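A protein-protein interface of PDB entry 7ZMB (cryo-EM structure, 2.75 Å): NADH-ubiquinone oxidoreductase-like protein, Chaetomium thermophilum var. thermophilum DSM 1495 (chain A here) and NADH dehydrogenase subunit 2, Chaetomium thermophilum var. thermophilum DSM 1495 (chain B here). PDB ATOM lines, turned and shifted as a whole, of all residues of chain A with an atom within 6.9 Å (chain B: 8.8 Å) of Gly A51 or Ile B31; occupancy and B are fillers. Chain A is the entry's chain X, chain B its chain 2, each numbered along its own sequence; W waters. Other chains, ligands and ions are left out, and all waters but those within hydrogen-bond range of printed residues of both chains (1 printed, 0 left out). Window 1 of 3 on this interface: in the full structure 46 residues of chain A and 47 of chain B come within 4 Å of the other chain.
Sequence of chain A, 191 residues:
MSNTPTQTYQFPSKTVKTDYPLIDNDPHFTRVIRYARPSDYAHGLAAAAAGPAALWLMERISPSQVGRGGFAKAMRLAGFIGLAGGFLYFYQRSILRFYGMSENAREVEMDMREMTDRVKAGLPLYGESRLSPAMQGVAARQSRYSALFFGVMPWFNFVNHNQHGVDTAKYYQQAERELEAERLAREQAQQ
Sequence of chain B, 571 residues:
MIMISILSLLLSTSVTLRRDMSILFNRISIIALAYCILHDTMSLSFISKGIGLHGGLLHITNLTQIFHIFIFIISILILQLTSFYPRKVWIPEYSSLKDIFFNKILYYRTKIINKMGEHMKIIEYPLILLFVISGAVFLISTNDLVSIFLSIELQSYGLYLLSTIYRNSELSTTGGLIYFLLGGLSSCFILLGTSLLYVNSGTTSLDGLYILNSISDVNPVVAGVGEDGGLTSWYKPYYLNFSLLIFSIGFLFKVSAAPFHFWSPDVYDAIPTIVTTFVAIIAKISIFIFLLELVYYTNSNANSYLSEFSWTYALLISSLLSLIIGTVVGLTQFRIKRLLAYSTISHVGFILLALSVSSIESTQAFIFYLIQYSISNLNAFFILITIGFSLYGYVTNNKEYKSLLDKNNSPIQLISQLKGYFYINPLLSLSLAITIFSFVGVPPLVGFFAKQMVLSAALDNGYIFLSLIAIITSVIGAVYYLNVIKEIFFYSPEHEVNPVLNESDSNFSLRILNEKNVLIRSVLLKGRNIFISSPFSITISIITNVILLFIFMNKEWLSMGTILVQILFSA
Of the 22 printed residues of chain B, 5 touch a printed residue of chain A.
Printed residues of chain A that touch a printed residue of chain B: Ala A47, Ala A48, Ala A50, Gly A51, Leu A55, Met A58, Ile A81 and Gly A82.
Hydrophobic or aromatic side chains of chain A within 4 Å of the printed part of chain B: Leu A55, Met A58 and Ile A81.
Among the printed residues, no Asp or Glu carboxylate lies within 4 Å of a Lys or Arg side-chain nitrogen of the other chain.
Water W1 lies within hydrogen-bond range of O of Leu A55 (2.9 Å) and NH2 of Arg B27 (3.0 Å).
Of the printed residues of chain A, Ile B31 touches Gly A51, Leu A55 and Met A58.
No residue of chain B comes within 4 Å of Pro A52.
Of the printed residues of chain B, Ile A81 touches Met B1 (3.6 Å), Ile B28 (3.7 Å) and Tyr B35 (3.98 Å).
Of the printed residues of chain B, Ala A50 touches Tyr B35.
Of the printed residues of chain B, Ala A48 touches Tyr B35.
Ile B30 touches none of the printed residues of chain A.
The nearest residue of chain A that does not touch Ile B31 is Ala A54 (4.1 Å).
The backbone carbonyl oxygen (O) of Ala A47 lies within hydrogen-bond range of the side-chain hydroxyl (OH) of Tyr B35 (2.5 Å).
The backbone NH (N) of Gly A51 is in hydrogen-bond range of the side-chain hydroxyl (OH) of Tyr B35 (3.0 Å).
OG of Ser B5 is in hydrogen-bond range of O of Met B1 (2.9 Å).
The backbone carbonyl oxygen (O) of Ser B83 is in hydrogen-bond range of the guanidinium group (NE) of Arg B27 (2.9 Å).
A ring nitrogen (ND1) of His B39 is in hydrogen-bond range of the backbone carbonyl oxygen (O) of Tyr B35, at 3.2 Å.
Among the printed residues, pairs that only touch across the chains: Gly A82 with Tyr B35, Gly A51 with Ile B31, Leu A55 with Arg B27, Ile A81 with Met B1, Met A58 with Arg B27, Ile A81 with Ile B28, Leu A55 with Ile B31, Ala A48 with Tyr B35, Leu A55 with Ile B28, Met A58 with Ile B31, Ile A81 with Tyr B35 and Ala A50 with Tyr B35.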
ATOM      1  N   ALA A  46       8.474 -11.906  11.905  1.00  0.00           N
ATOM      2  CA  ALA A  46       9.067 -12.287  13.209  1.00  0.00           C
ATOM      3  C   ALA A  46       8.425 -13.573  13.727  1.00  0.00           C
ATOM      4  O   ALA A  46       9.160 -14.421  14.245  1.00  0.00           O
ATOM      5  CB  ALA A  46       8.871 -11.160  14.195  1.00  0.00           C
ATOM      6  N   ALA A  47       7.104 -13.699  13.596  1.00  0.00           N
ATOM      7  CA  ALA A  47       6.370 -14.896  14.052  1.00  0.00           C
ATOM      8  C   ALA A  47       6.828 -16.126  13.268  1.00  0.00           C
ATOM      9  O   ALA A  47       7.026 -17.176  13.901  1.00  0.00           O
ATOM     10  CB  ALA A  47       4.893 -14.649  13.879  1.00  0.00           C
ATOM     11  N   ALA A  48       7.016 -16.001  11.954  1.00  0.00           N
ATOM     12  CA  ALA A  48       7.526 -17.128  11.144  1.00  0.00           C
ATOM     13  C   ALA A  48       8.937 -17.514  11.603  1.00  0.00           C
ATOM     14  O   ALA A  48       9.225 -18.722  11.675  1.00  0.00           O
ATOM     15  CB  ALA A  48       7.471 -16.791   9.679  1.00  0.00           C
ATOM     16  N   ALA A  49       9.781 -16.532  11.902  1.00  0.00           N
ATOM     17  CA  ALA A  49      11.142 -16.814  12.410  1.00  0.00           C
ATOM     18  C   ALA A  49      11.076 -17.474  13.789  1.00  0.00           C
ATOM     19  O   ALA A  49      11.965 -18.281  14.080  1.00  0.00           O
ATOM     20  CB  ALA A  49      11.944 -15.543  12.448  1.00  0.00           C
ATOM     21  N   ALA A  50      10.047 -17.180  14.584  1.00  0.00           N
ATOM     22  CA  ALA A  50       9.997 -17.654  15.988  1.00  0.00           C
ATOM     23  C   ALA A  50      10.034 -19.177  16.107  1.00  0.00           C
ATOM     24  O   ALA A  50      10.699 -19.645  17.038  1.00  0.00           O
ATOM     25  CB  ALA A  50       8.791 -17.076  16.683  1.00  0.00           C
ATOM     26  N   GLY A  51       9.355 -19.916  15.227  1.00  0.00           N
ATOM     27  CA  GLY A  51       9.271 -21.375  15.410  1.00  0.00           C
ATOM     28  C   GLY A  51      10.592 -22.078  15.151  1.00  0.00           C
ATOM     29  O   GLY A  51      11.053 -22.761  16.074  1.00  0.00           O
ATOM     30  N   PRO A  52      11.253 -21.998  13.971  1.00  0.00           N
ATOM     31  CA  PRO A  52      12.567 -22.641  13.829  1.00  0.00           C
ATOM     32  C   PRO A  52      13.628 -22.056  14.748  1.00  0.00           C
ATOM     33  O   PRO A  52      14.567 -22.765  15.129  1.00  0.00           O
ATOM     34  CB  PRO A  52      12.899 -22.424  12.349  1.00  0.00           C
ATOM     35  CG  PRO A  52      12.077 -21.280  11.942  1.00  0.00           C
ATOM     36  CD  PRO A  52      10.815 -21.379  12.713  1.00  0.00           C
ATOM     37  N   ALA A  53      13.518 -20.775  15.101  1.00  0.00           N
ATOM     38  CA  ALA A  53      14.430 -20.226  16.090  1.00  0.00           C
ATOM     39  C   ALA A  53      14.191 -20.845  17.454  1.00  0.00           C
ATOM     40  O   ALA A  53      15.125 -20.966  18.251  1.00  0.00           O
ATOM     41  CB  ALA A  53      14.297 -18.707  16.161  1.00  0.00           C
ATOM     42  N   ALA A  54      12.953 -21.242  17.740  1.00  0.00           N
ATOM     43  CA  ALA A  54      12.675 -21.938  18.989  1.00  0.00           C
ATOM     44  C   ALA A  54      13.290 -23.330  18.984  1.00  0.00           C
ATOM     45  O   ALA A  54      13.939 -23.733  19.953  1.00  0.00           O
ATOM     46  CB  ALA A  54      11.168 -22.003  19.228  1.00  0.00           C
ATOM     47  N   LEU A  55      13.111 -24.072  17.887  1.00  0.00           N
ATOM     48  CA  LEU A  55      13.667 -25.418  17.791  1.00  0.00           C
ATOM     49  C   LEU A  55      15.187 -25.396  17.736  1.00  0.00           C
ATOM     50  O   LEU A  55      15.835 -26.356  18.155  1.00  0.00           O
ATOM     51  CB  LEU A  55      13.092 -26.140  16.571  1.00  0.00           C
ATOM     52  CG  LEU A  55      13.341 -27.648  16.413  1.00  0.00           C
ATOM     53  CD1 LEU A  55      12.561 -28.467  17.423  1.00  0.00           C
ATOM     54  CD2 LEU A  55      13.022 -28.114  15.011  1.00  0.00           C
ATOM     55  N   TRP A  56      15.778 -24.299  17.277  1.00  0.00           N
ATOM     56  CA  TRP A  56      17.260 -24.130  17.307  1.00  0.00           C
ATOM     57  C   TRP A  56      17.744 -23.969  18.750  1.00  0.00           C
ATOM     58  O   TRP A  56      18.725 -24.618  19.106  1.00  0.00           O
ATOM     59  CB  TRP A  56      17.748 -22.977  16.428  1.00  0.00           C
ATOM     60  CG  TRP A  56      19.239 -22.956  16.297  1.00  0.00           C
ATOM     61  CD1 TRP A  56      19.992 -23.630  15.380  1.00  0.00           C
ATOM     62  CD2 TRP A  56      20.170 -22.244  17.132  1.00  0.00           C
ATOM     63  NE1 TRP A  56      21.322 -23.378  15.579  1.00  0.00           N
ATOM     64  CE2 TRP A  56      21.462 -22.534  16.649  1.00  0.00           C
ATOM     65  CE3 TRP A  56      20.039 -21.394  18.236  1.00  0.00           C
ATOM     66  CZ2 TRP A  56      22.611 -22.001  17.232  1.00  0.00           C
ATOM     67  CZ3 TRP A  56      21.174 -20.872  18.813  1.00  0.00           C
ATOM     68  CH2 TRP A  56      22.441 -21.170  18.315  1.00  0.00           C
ATOM     69  N   MET A  58      16.247 -24.837  21.507  1.00  0.00           N
ATOM     70  CA  MET A  58      16.011 -26.104  22.243  1.00  0.00           C
ATOM     71  C   MET A  58      17.135 -27.070  21.892  1.00  0.00           C
ATOM     72  O   MET A  58      17.580 -27.795  22.784  1.00  0.00           O
ATOM     73  CB  MET A  58      14.651 -26.728  21.922  1.00  0.00           C
ATOM     74  CG  MET A  58      13.510 -26.137  22.727  1.00  0.00           C
ATOM     75  SD  MET A  58      11.900 -26.873  22.347  1.00  0.00           S
ATOM     76  CE  MET A  58      11.518 -26.077  20.790  1.00  0.00           C
ATOM     77  N   MET A  75      14.097 -29.054  10.960  1.00  0.00           N
ATOM     78  CA  MET A  75      14.086 -27.637  10.624  1.00  0.00           C
ATOM     79  C   MET A  75      13.119 -27.348   9.488  1.00  0.00           C
ATOM     80  O   MET A  75      12.382 -26.358   9.525  1.00  0.00           O
ATOM     81  CB  MET A  75      15.495 -27.181  10.258  1.00  0.00           C
ATOM     82  CG  MET A  75      16.285 -26.592  11.393  1.00  0.00           C
ATOM     83  SD  MET A  75      15.583 -25.063  12.030  1.00  0.00           S
ATOM     84  CE  MET A  75      15.014 -25.596  13.624  1.00  0.00           C
ATOM     85  N   ALA A  78       9.707 -27.372  10.997  1.00  0.00           N
ATOM     86  CA  ALA A  78       9.567 -26.185  11.829  1.00  0.00           C
ATOM     87  C   ALA A  78       9.587 -24.920  10.984  1.00  0.00           C
ATOM     88  O   ALA A  78       8.878 -23.956  11.281  1.00  0.00           O
ATOM     89  CB  ALA A  78      10.667 -26.144  12.886  1.00  0.00           C
ATOM     90  N   GLY A  79      10.399 -24.910   9.930  1.00  0.00           N
ATOM     91  CA  GLY A  79      10.404 -23.770   9.034  1.00  0.00           C
ATOM     92  C   GLY A  79       9.057 -23.547   8.378  1.00  0.00           C
ATOM     93  O   GLY A  79       8.568 -22.421   8.305  1.00  0.00           O
ATOM     94  N   ILE A  81       5.991 -24.714   9.403  1.00  0.00           N
ATOM     95  CA  ILE A  81       4.948 -24.433  10.385  1.00  0.00           C
ATOM     96  C   ILE A  81       5.062 -23.001  10.895  1.00  0.00           C
ATOM     97  O   ILE A  81       4.054 -22.341  11.159  1.00  0.00           O
ATOM     98  CB  ILE A  81       4.999 -25.470  11.525  1.00  0.00           C
ATOM     99  CG1 ILE A  81       4.503 -26.827  11.020  1.00  0.00           C
ATOM    100  CG2 ILE A  81       4.208 -25.026  12.751  1.00  0.00           C
ATOM    101  CD1 ILE A  81       4.687 -27.935  11.981  1.00  0.00           C
ATOM    102  N   GLY A  82       6.276 -22.474  10.980  1.00  0.00           N
ATOM    103  CA  GLY A  82       6.354 -21.070  11.394  1.00  0.00           C
ATOM    104  C   GLY A  82       5.932 -20.162  10.267  1.00  0.00           C
ATOM    105  O   GLY A  82       5.220 -19.202  10.553  1.00  0.00           O
ATOM    106  N   MET B   1      -4.891 -23.647  12.011  1.00  0.00           N
ATOM    107  CA  MET B   1      -3.499 -23.837  12.409  1.00  0.00           C
ATOM    108  C   MET B   1      -3.279 -25.253  12.939  1.00  0.00           C
ATOM    109  O   MET B   1      -2.314 -25.903  12.578  1.00  0.00           O
ATOM    110  CB  MET B   1      -3.086 -22.798  13.456  1.00  0.00           C
ATOM    111  CG  MET B   1      -1.587 -22.730  13.733  1.00  0.00           C
ATOM    112  SD  MET B   1      -0.570 -22.750  12.243  1.00  0.00           S
ATOM    113  CE  MET B   1       0.851 -23.674  12.780  1.00  0.00           C
ATOM    114  N   SER B   5      -1.049 -27.970  11.156  1.00  0.00           N
ATOM    115  CA  SER B   5       0.016 -28.596  11.923  1.00  0.00           C
ATOM    116  C   SER B   5      -0.082 -30.113  11.874  1.00  0.00           C
ATOM    117  O   SER B   5       0.942 -30.799  11.840  1.00  0.00           O
ATOM    118  CB  SER B   5      -0.009 -28.094  13.361  1.00  0.00           C
ATOM    119  OG  SER B   5       0.379 -26.739  13.421  1.00  0.00           O
ATOM    120  N   LEU B  24      12.116 -34.890  18.311  1.00  0.00           N
ATOM    121  CA  LEU B  24      12.067 -33.609  17.567  1.00  0.00           C
ATOM    122  C   LEU B  24      10.654 -33.399  17.025  1.00  0.00           C
ATOM    123  O   LEU B  24      10.240 -32.244  16.990  1.00  0.00           O
ATOM    124  CB  LEU B  24      13.129 -33.631  16.463  1.00  0.00           C
ATOM    125  CG  LEU B  24      14.565 -33.354  16.893  1.00  0.00           C
ATOM    126  CD1 LEU B  24      15.517 -33.667  15.754  1.00  0.00           C
ATOM    127  CD2 LEU B  24      14.726 -31.911  17.339  1.00  0.00           C
ATOM    128  N   PHE B  25       9.925 -34.467  16.670  1.00  0.00           N
ATOM    129  CA  PHE B  25       8.525 -34.304  16.290  1.00  0.00           C
ATOM    130  C   PHE B  25       7.684 -33.825  17.463  1.00  0.00           C
ATOM    131  O   PHE B  25       6.681 -33.133  17.266  1.00  0.00           O
ATOM    132  CB  PHE B  25       7.969 -35.616  15.738  1.00  0.00           C
ATOM    133  CG  PHE B  25       8.339 -35.874  14.311  1.00  0.00           C
ATOM    134  CD1 PHE B  25       8.783 -34.847  13.502  1.00  0.00           C
ATOM    135  CD2 PHE B  25       8.241 -37.138  13.774  1.00  0.00           C
ATOM    136  CE1 PHE B  25       9.126 -35.077  12.201  1.00  0.00           C
ATOM    137  CE2 PHE B  25       8.586 -37.370  12.459  1.00  0.00           C
ATOM    138  CZ  PHE B  25       9.030 -36.338  11.676  1.00  0.00           C
ATOM    139  N   ASN B  26       8.082 -34.151  18.693  1.00  0.00           N
ATOM    140  CA  ASN B  26       7.346 -33.648  19.885  1.00  0.00           C
ATOM    141  C   ASN B  26       7.690 -32.171  20.115  1.00  0.00           C
ATOM    142  O   ASN B  26       6.782 -31.419  20.492  1.00  0.00           O
ATOM    143  CB  ASN B  26       7.562 -34.536  21.114  1.00  0.00           C
ATOM    144  CG  ASN B  26       6.721 -35.791  21.125  1.00  0.00           C
ATOM    145  OD1 ASN B  26       5.564 -35.761  21.529  1.00  0.00           O
ATOM    146  ND2 ASN B  26       7.302 -36.907  20.727  1.00  0.00           N
ATOM    147  N   ARG B  27       8.943 -31.780  19.891  1.00  0.00           N
ATOM    148  CA  ARG B  27       9.402 -30.375  20.082  1.00  0.00           C
ATOM    149  C   ARG B  27       8.744 -29.440  19.065  1.00  0.00           C
ATOM    150  O   ARG B  27       8.532 -28.269  19.401  1.00  0.00           O
ATOM    151  CB  ARG B  27      10.927 -30.286  20.066  1.00  0.00           C
ATOM    152  CG  ARG B  27      11.597 -30.671  21.376  1.00  0.00           C
ATOM    153  CD  ARG B  27      13.104 -30.603  21.249  1.00  0.00           C
ATOM    154  NE  ARG B  27      13.776 -30.989  22.479  1.00  0.00           N
ATOM    155  CZ  ARG B  27      15.091 -31.068  22.625  1.00  0.00           C
ATOM    156  NH1 ARG B  27      15.603 -31.432  23.788  1.00  0.00           N
ATOM    157  NH2 ARG B  27      15.888 -30.783  21.613  1.00  0.00           N
ATOM    158  N   ILE B  28       8.407 -29.956  17.885  1.00  0.00           N
ATOM    159  CA  ILE B  28       7.794 -29.134  16.807  1.00  0.00           C
ATOM    160  C   ILE B  28       6.307 -29.000  17.123  1.00  0.00           C
ATOM    161  O   ILE B  28       5.734 -27.939  16.842  1.00  0.00           O
ATOM    162  CB  ILE B  28       8.050 -29.772  15.424  1.00  0.00           C
ATOM    163  CG1 ILE B  28       9.534 -29.748  15.060  1.00  0.00           C
ATOM    164  CG2 ILE B  28       7.209 -29.117  14.341  1.00  0.00           C
ATOM    165  CD1 ILE B  28       9.872 -30.599  13.868  1.00  0.00           C
ATOM    166  N   SER B  29       5.728 -30.018  17.751  1.00  0.00           N
ATOM    167  CA  SER B  29       4.320 -29.935  18.119  1.00  0.00           C
ATOM    168  C   SER B  29       4.068 -28.864  19.175  1.00  0.00           C
ATOM    169  O   SER B  29       3.013 -28.221  19.165  1.00  0.00           O
ATOM    170  CB  SER B  29       3.840 -31.293  18.613  1.00  0.00           C
ATOM    171  OG  SER B  29       3.924 -32.252  17.584  1.00  0.00           O
ATOM    172  N   ILE B  30       5.018 -28.664  20.092  1.00  0.00           N
ATOM    173  CA  ILE B  30       4.906 -27.583  21.065  1.00  0.00           C
ATOM    174  C   ILE B  30       4.996 -26.223  20.376  1.00  0.00           C
ATOM    175  O   ILE B  30       4.278 -25.283  20.735  1.00  0.00           O
ATOM    176  CB  ILE B  30       5.962 -27.754  22.174  1.00  0.00           C
ATOM    177  CG1 ILE B  30       5.565 -28.910  23.094  1.00  0.00           C
ATOM    178  CG2 ILE B  30       6.131 -26.481  22.980  1.00  0.00           C
ATOM    179  CD1 ILE B  30       6.619 -29.317  24.076  1.00  0.00           C
ATOM    180  N   ILE B  31       5.857 -26.098  19.366  1.00  0.00           N
ATOM    181  CA  ILE B  31       5.892 -24.875  18.570  1.00  0.00           C
ATOM    182  C   ILE B  31       4.558 -24.658  17.859  1.00  0.00           C
ATOM    183  O   ILE B  31       4.032 -23.542  17.821  1.00  0.00           O
ATOM    184  CB  ILE B  31       7.071 -24.919  17.581  1.00  0.00           C
ATOM    185  CG1 ILE B  31       8.399 -24.947  18.341  1.00  0.00           C
ATOM    186  CG2 ILE B  31       7.018 -23.748  16.642  1.00  0.00           C
ATOM    187  CD1 ILE B  31       9.589 -25.348  17.500  1.00  0.00           C
ATOM    188  N   ALA B  32       3.970 -25.728  17.335  1.00  0.00           N
ATOM    189  CA  ALA B  32       2.690 -25.615  16.602  1.00  0.00           C
ATOM    190  C   ALA B  32       1.560 -25.138  17.522  1.00  0.00           C
ATOM    191  O   ALA B  32       0.791 -24.268  17.086  1.00  0.00           O
ATOM    192  CB  ALA B  32       2.364 -26.933  15.959  1.00  0.00           C
ATOM    193  N   LEU B  33       1.456 -25.690  18.733  1.00  0.00           N
ATOM    194  CA  LEU B  33       0.379 -25.331  19.690  1.00  0.00           C
ATOM    195  C   LEU B  33       0.570 -23.899  20.184  1.00  0.00           C
ATOM    196  O   LEU B  33      -0.427 -23.296  20.609  1.00  0.00           O
ATOM    197  CB  LEU B  33       0.376 -26.339  20.839  1.00  0.00           C
ATOM    198  CG  LEU B  33      -0.131 -27.734  20.491  1.00  0.00           C
ATOM    199  CD1 LEU B  33       0.254 -28.731  21.570  1.00  0.00           C
ATOM    200  CD2 LEU B  33      -1.635 -27.719  20.292  1.00  0.00           C
ATOM    201  N   ALA B  34       1.794 -23.373  20.095  1.00  0.00           N
ATOM    202  CA  ALA B  34       2.077 -21.991  20.527  1.00  0.00           C
ATOM    203  C   ALA B  34       1.553 -21.029  19.462  1.00  0.00           C
ATOM    204  O   ALA B  34       1.149 -19.914  19.825  1.00  0.00           O
ATOM    205  CB  ALA B  34       3.556 -21.822  20.715  1.00  0.00           C
ATOM    206  N   TYR B  35       1.505 -21.452  18.194  1.00  0.00           N
ATOM    207  CA  TYR B  35       0.932 -20.593  17.126  1.00  0.00           C
ATOM    208  C   TYR B  35      -0.578 -20.571  17.284  1.00  0.00           C
ATOM    209  O   TYR B  35      -1.179 -19.505  17.125  1.00  0.00           O
ATOM    210  CB  TYR B  35       1.333 -21.060  15.727  1.00  0.00           C
ATOM    211  CG  TYR B  35       2.724 -20.671  15.309  1.00  0.00           C
ATOM    212  CD1 TYR B  35       3.026 -19.364  14.970  1.00  0.00           C
ATOM    213  CD2 TYR B  35       3.735 -21.611  15.248  1.00  0.00           C
ATOM    214  CE1 TYR B  35       4.304 -18.999  14.584  1.00  0.00           C
ATOM    215  CE2 TYR B  35       5.018 -21.264  14.867  1.00  0.00           C
ATOM    216  CZ  TYR B  35       5.303 -19.954  14.536  1.00  0.00           C
ATOM    217  OH  TYR B  35       6.568 -19.611  14.165  1.00  0.00           O
ATOM    218  N   CYS B  36      -1.155 -21.719  17.624  1.00  0.00           N
ATOM    219  CA  CYS B  36      -2.590 -21.755  17.876  1.00  0.00           C
ATOM    220  C   CYS B  36      -2.976 -20.807  19.004  1.00  0.00           C
ATOM    221  O   CYS B  36      -4.045 -20.189  18.966  1.00  0.00           O
ATOM    222  CB  CYS B  36      -3.022 -23.181  18.211  1.00  0.00           C
ATOM    223  SG  CYS B  36      -2.820 -24.380  16.892  1.00  0.00           S
ATOM    224  N   ILE B  37      -2.127 -20.698  20.026  1.00  0.00           N
ATOM    225  CA  ILE B  37      -2.377 -19.758  21.113  1.00  0.00           C
ATOM    226  C   ILE B  37      -2.337 -18.321  20.603  1.00  0.00           C
ATOM    227  O   ILE B  37      -3.186 -17.497  20.963  1.00  0.00           O
ATOM    228  CB  ILE B  37      -1.372 -19.997  22.256  1.00  0.00           C
ATOM    229  CG1 ILE B  37      -1.747 -21.268  23.018  1.00  0.00           C
ATOM    230  CG2 ILE B  37      -1.322 -18.813  23.198  1.00  0.00           C
ATOM    231  CD1 ILE B  37      -0.631 -21.884  23.817  1.00  0.00           C
ATOM    232  N   LEU B  38      -1.371 -17.998  19.743  1.00  0.00           N
ATOM    233  CA  LEU B  38      -1.228 -16.625  19.183  1.00  0.00           C
ATOM    234  C   LEU B  38      -2.449 -16.281  18.327  1.00  0.00           C
ATOM    235  O   LEU B  38      -2.837 -15.104  18.312  1.00  0.00           O
ATOM    236  CB  LEU B  38       0.062 -16.569  18.360  1.00  0.00           C
ATOM    237  CG  LEU B  38       0.438 -15.213  17.768  1.00  0.00           C
ATOM    238  CD1 LEU B  38       0.772 -14.214  18.866  1.00  0.00           C
ATOM    239  CD2 LEU B  38       1.612 -15.356  16.812  1.00  0.00           C
ATOM    240  N   HIS B  39      -3.049 -17.282  17.678  1.00  0.00           N
ATOM    241  CA  HIS B  39      -4.197 -17.030  16.819  1.00  0.00           C
ATOM    242  C   HIS B  39      -5.484 -16.874  17.620  1.00  0.00           C
ATOM    243  O   HIS B  39      -6.281 -15.968  17.350  1.00  0.00           O
ATOM    244  CB  HIS B  39      -4.313 -18.143  15.785  1.00  0.00           C
ATOM    245  CG  HIS B  39      -3.139 -18.216  14.862  1.00  0.00           C
ATOM    246  ND1 HIS B  39      -2.682 -19.396  14.322  1.00  0.00           N
ATOM    247  CD2 HIS B  39      -2.326 -17.245  14.383  1.00  0.00           C
ATOM    248  CE1 HIS B  39      -1.637 -19.151  13.556  1.00  0.00           C
ATOM    249  NE2 HIS B  39      -1.400 -17.854  13.576  1.00  0.00           N
ATOM    250  N   ILE B  76       0.738 -28.135  25.739  1.00  0.00           N
ATOM    251  CA  ILE B  76       2.158 -27.816  25.675  1.00  0.00           C
ATOM    252  C   ILE B  76       2.885 -28.361  26.897  1.00  0.00           C
ATOM    253  O   ILE B  76       3.992 -28.898  26.792  1.00  0.00           O
ATOM    254  CB  ILE B  76       2.345 -26.297  25.517  1.00  0.00           C
ATOM    255  CG1 ILE B  76       2.091 -25.895  24.066  1.00  0.00           C
ATOM    256  CG2 ILE B  76       3.727 -25.861  25.971  1.00  0.00           C
ATOM    257  CD1 ILE B  76       2.033 -24.430  23.843  1.00  0.00           C
ATOM    258  N   LEU B  79       3.042 -32.109  26.644  1.00  0.00           N
ATOM    259  CA  LEU B  79       3.890 -32.523  25.500  1.00  0.00           C
ATOM    260  C   LEU B  79       5.362 -32.469  25.904  1.00  0.00           C
ATOM    261  O   LEU B  79       6.178 -33.047  25.177  1.00  0.00           O
ATOM    262  CB  LEU B  79       3.579 -31.657  24.279  1.00  0.00           C
ATOM    263  CG  LEU B  79       3.627 -32.358  22.927  1.00  0.00           C
ATOM    264  CD1 LEU B  79       3.090 -33.775  23.030  1.00  0.00           C
ATOM    265  CD2 LEU B  79       2.838 -31.553  21.913  1.00  0.00           C
ATOM    266  N   SER B  83       9.184 -34.453  24.969  1.00  0.00           N
ATOM    267  CA  SER B  83      10.004 -33.475  24.201  1.00  0.00           C
ATOM    268  C   SER B  83      11.412 -33.331  24.782  1.00  0.00           C
ATOM    269  O   SER B  83      12.297 -32.884  24.051  1.00  0.00           O
ATOM    270  CB  SER B  83       9.310 -32.156  24.073  1.00  0.00           C
ATOM    271  OG  SER B  83       8.057 -32.305  23.433  1.00  0.00           O
ATOM    272  N   LEU B 130      -2.334 -34.459  18.764  1.00  0.00           N
ATOM    273  CA  LEU B 130      -2.850 -33.260  18.050  1.00  0.00           C
ATOM    274  C   LEU B 130      -4.264 -33.530  17.531  1.00  0.00           C
ATOM    275  O   LEU B 130      -5.070 -32.596  17.549  1.00  0.00           O
ATOM    276  CB  LEU B 130      -1.905 -32.886  16.907  1.00  0.00           C
ATOM    277  CG  LEU B 130      -0.568 -32.263  17.302  1.00  0.00           C
ATOM    278  CD1 LEU B 130       0.228 -31.887  16.065  1.00  0.00           C
ATOM    279  CD2 LEU B 130      -0.771 -31.043  18.186  1.00  0.00           C
HETATM  280  O   HOH W   1      15.334 -28.906  19.335  1.00  0.00           O
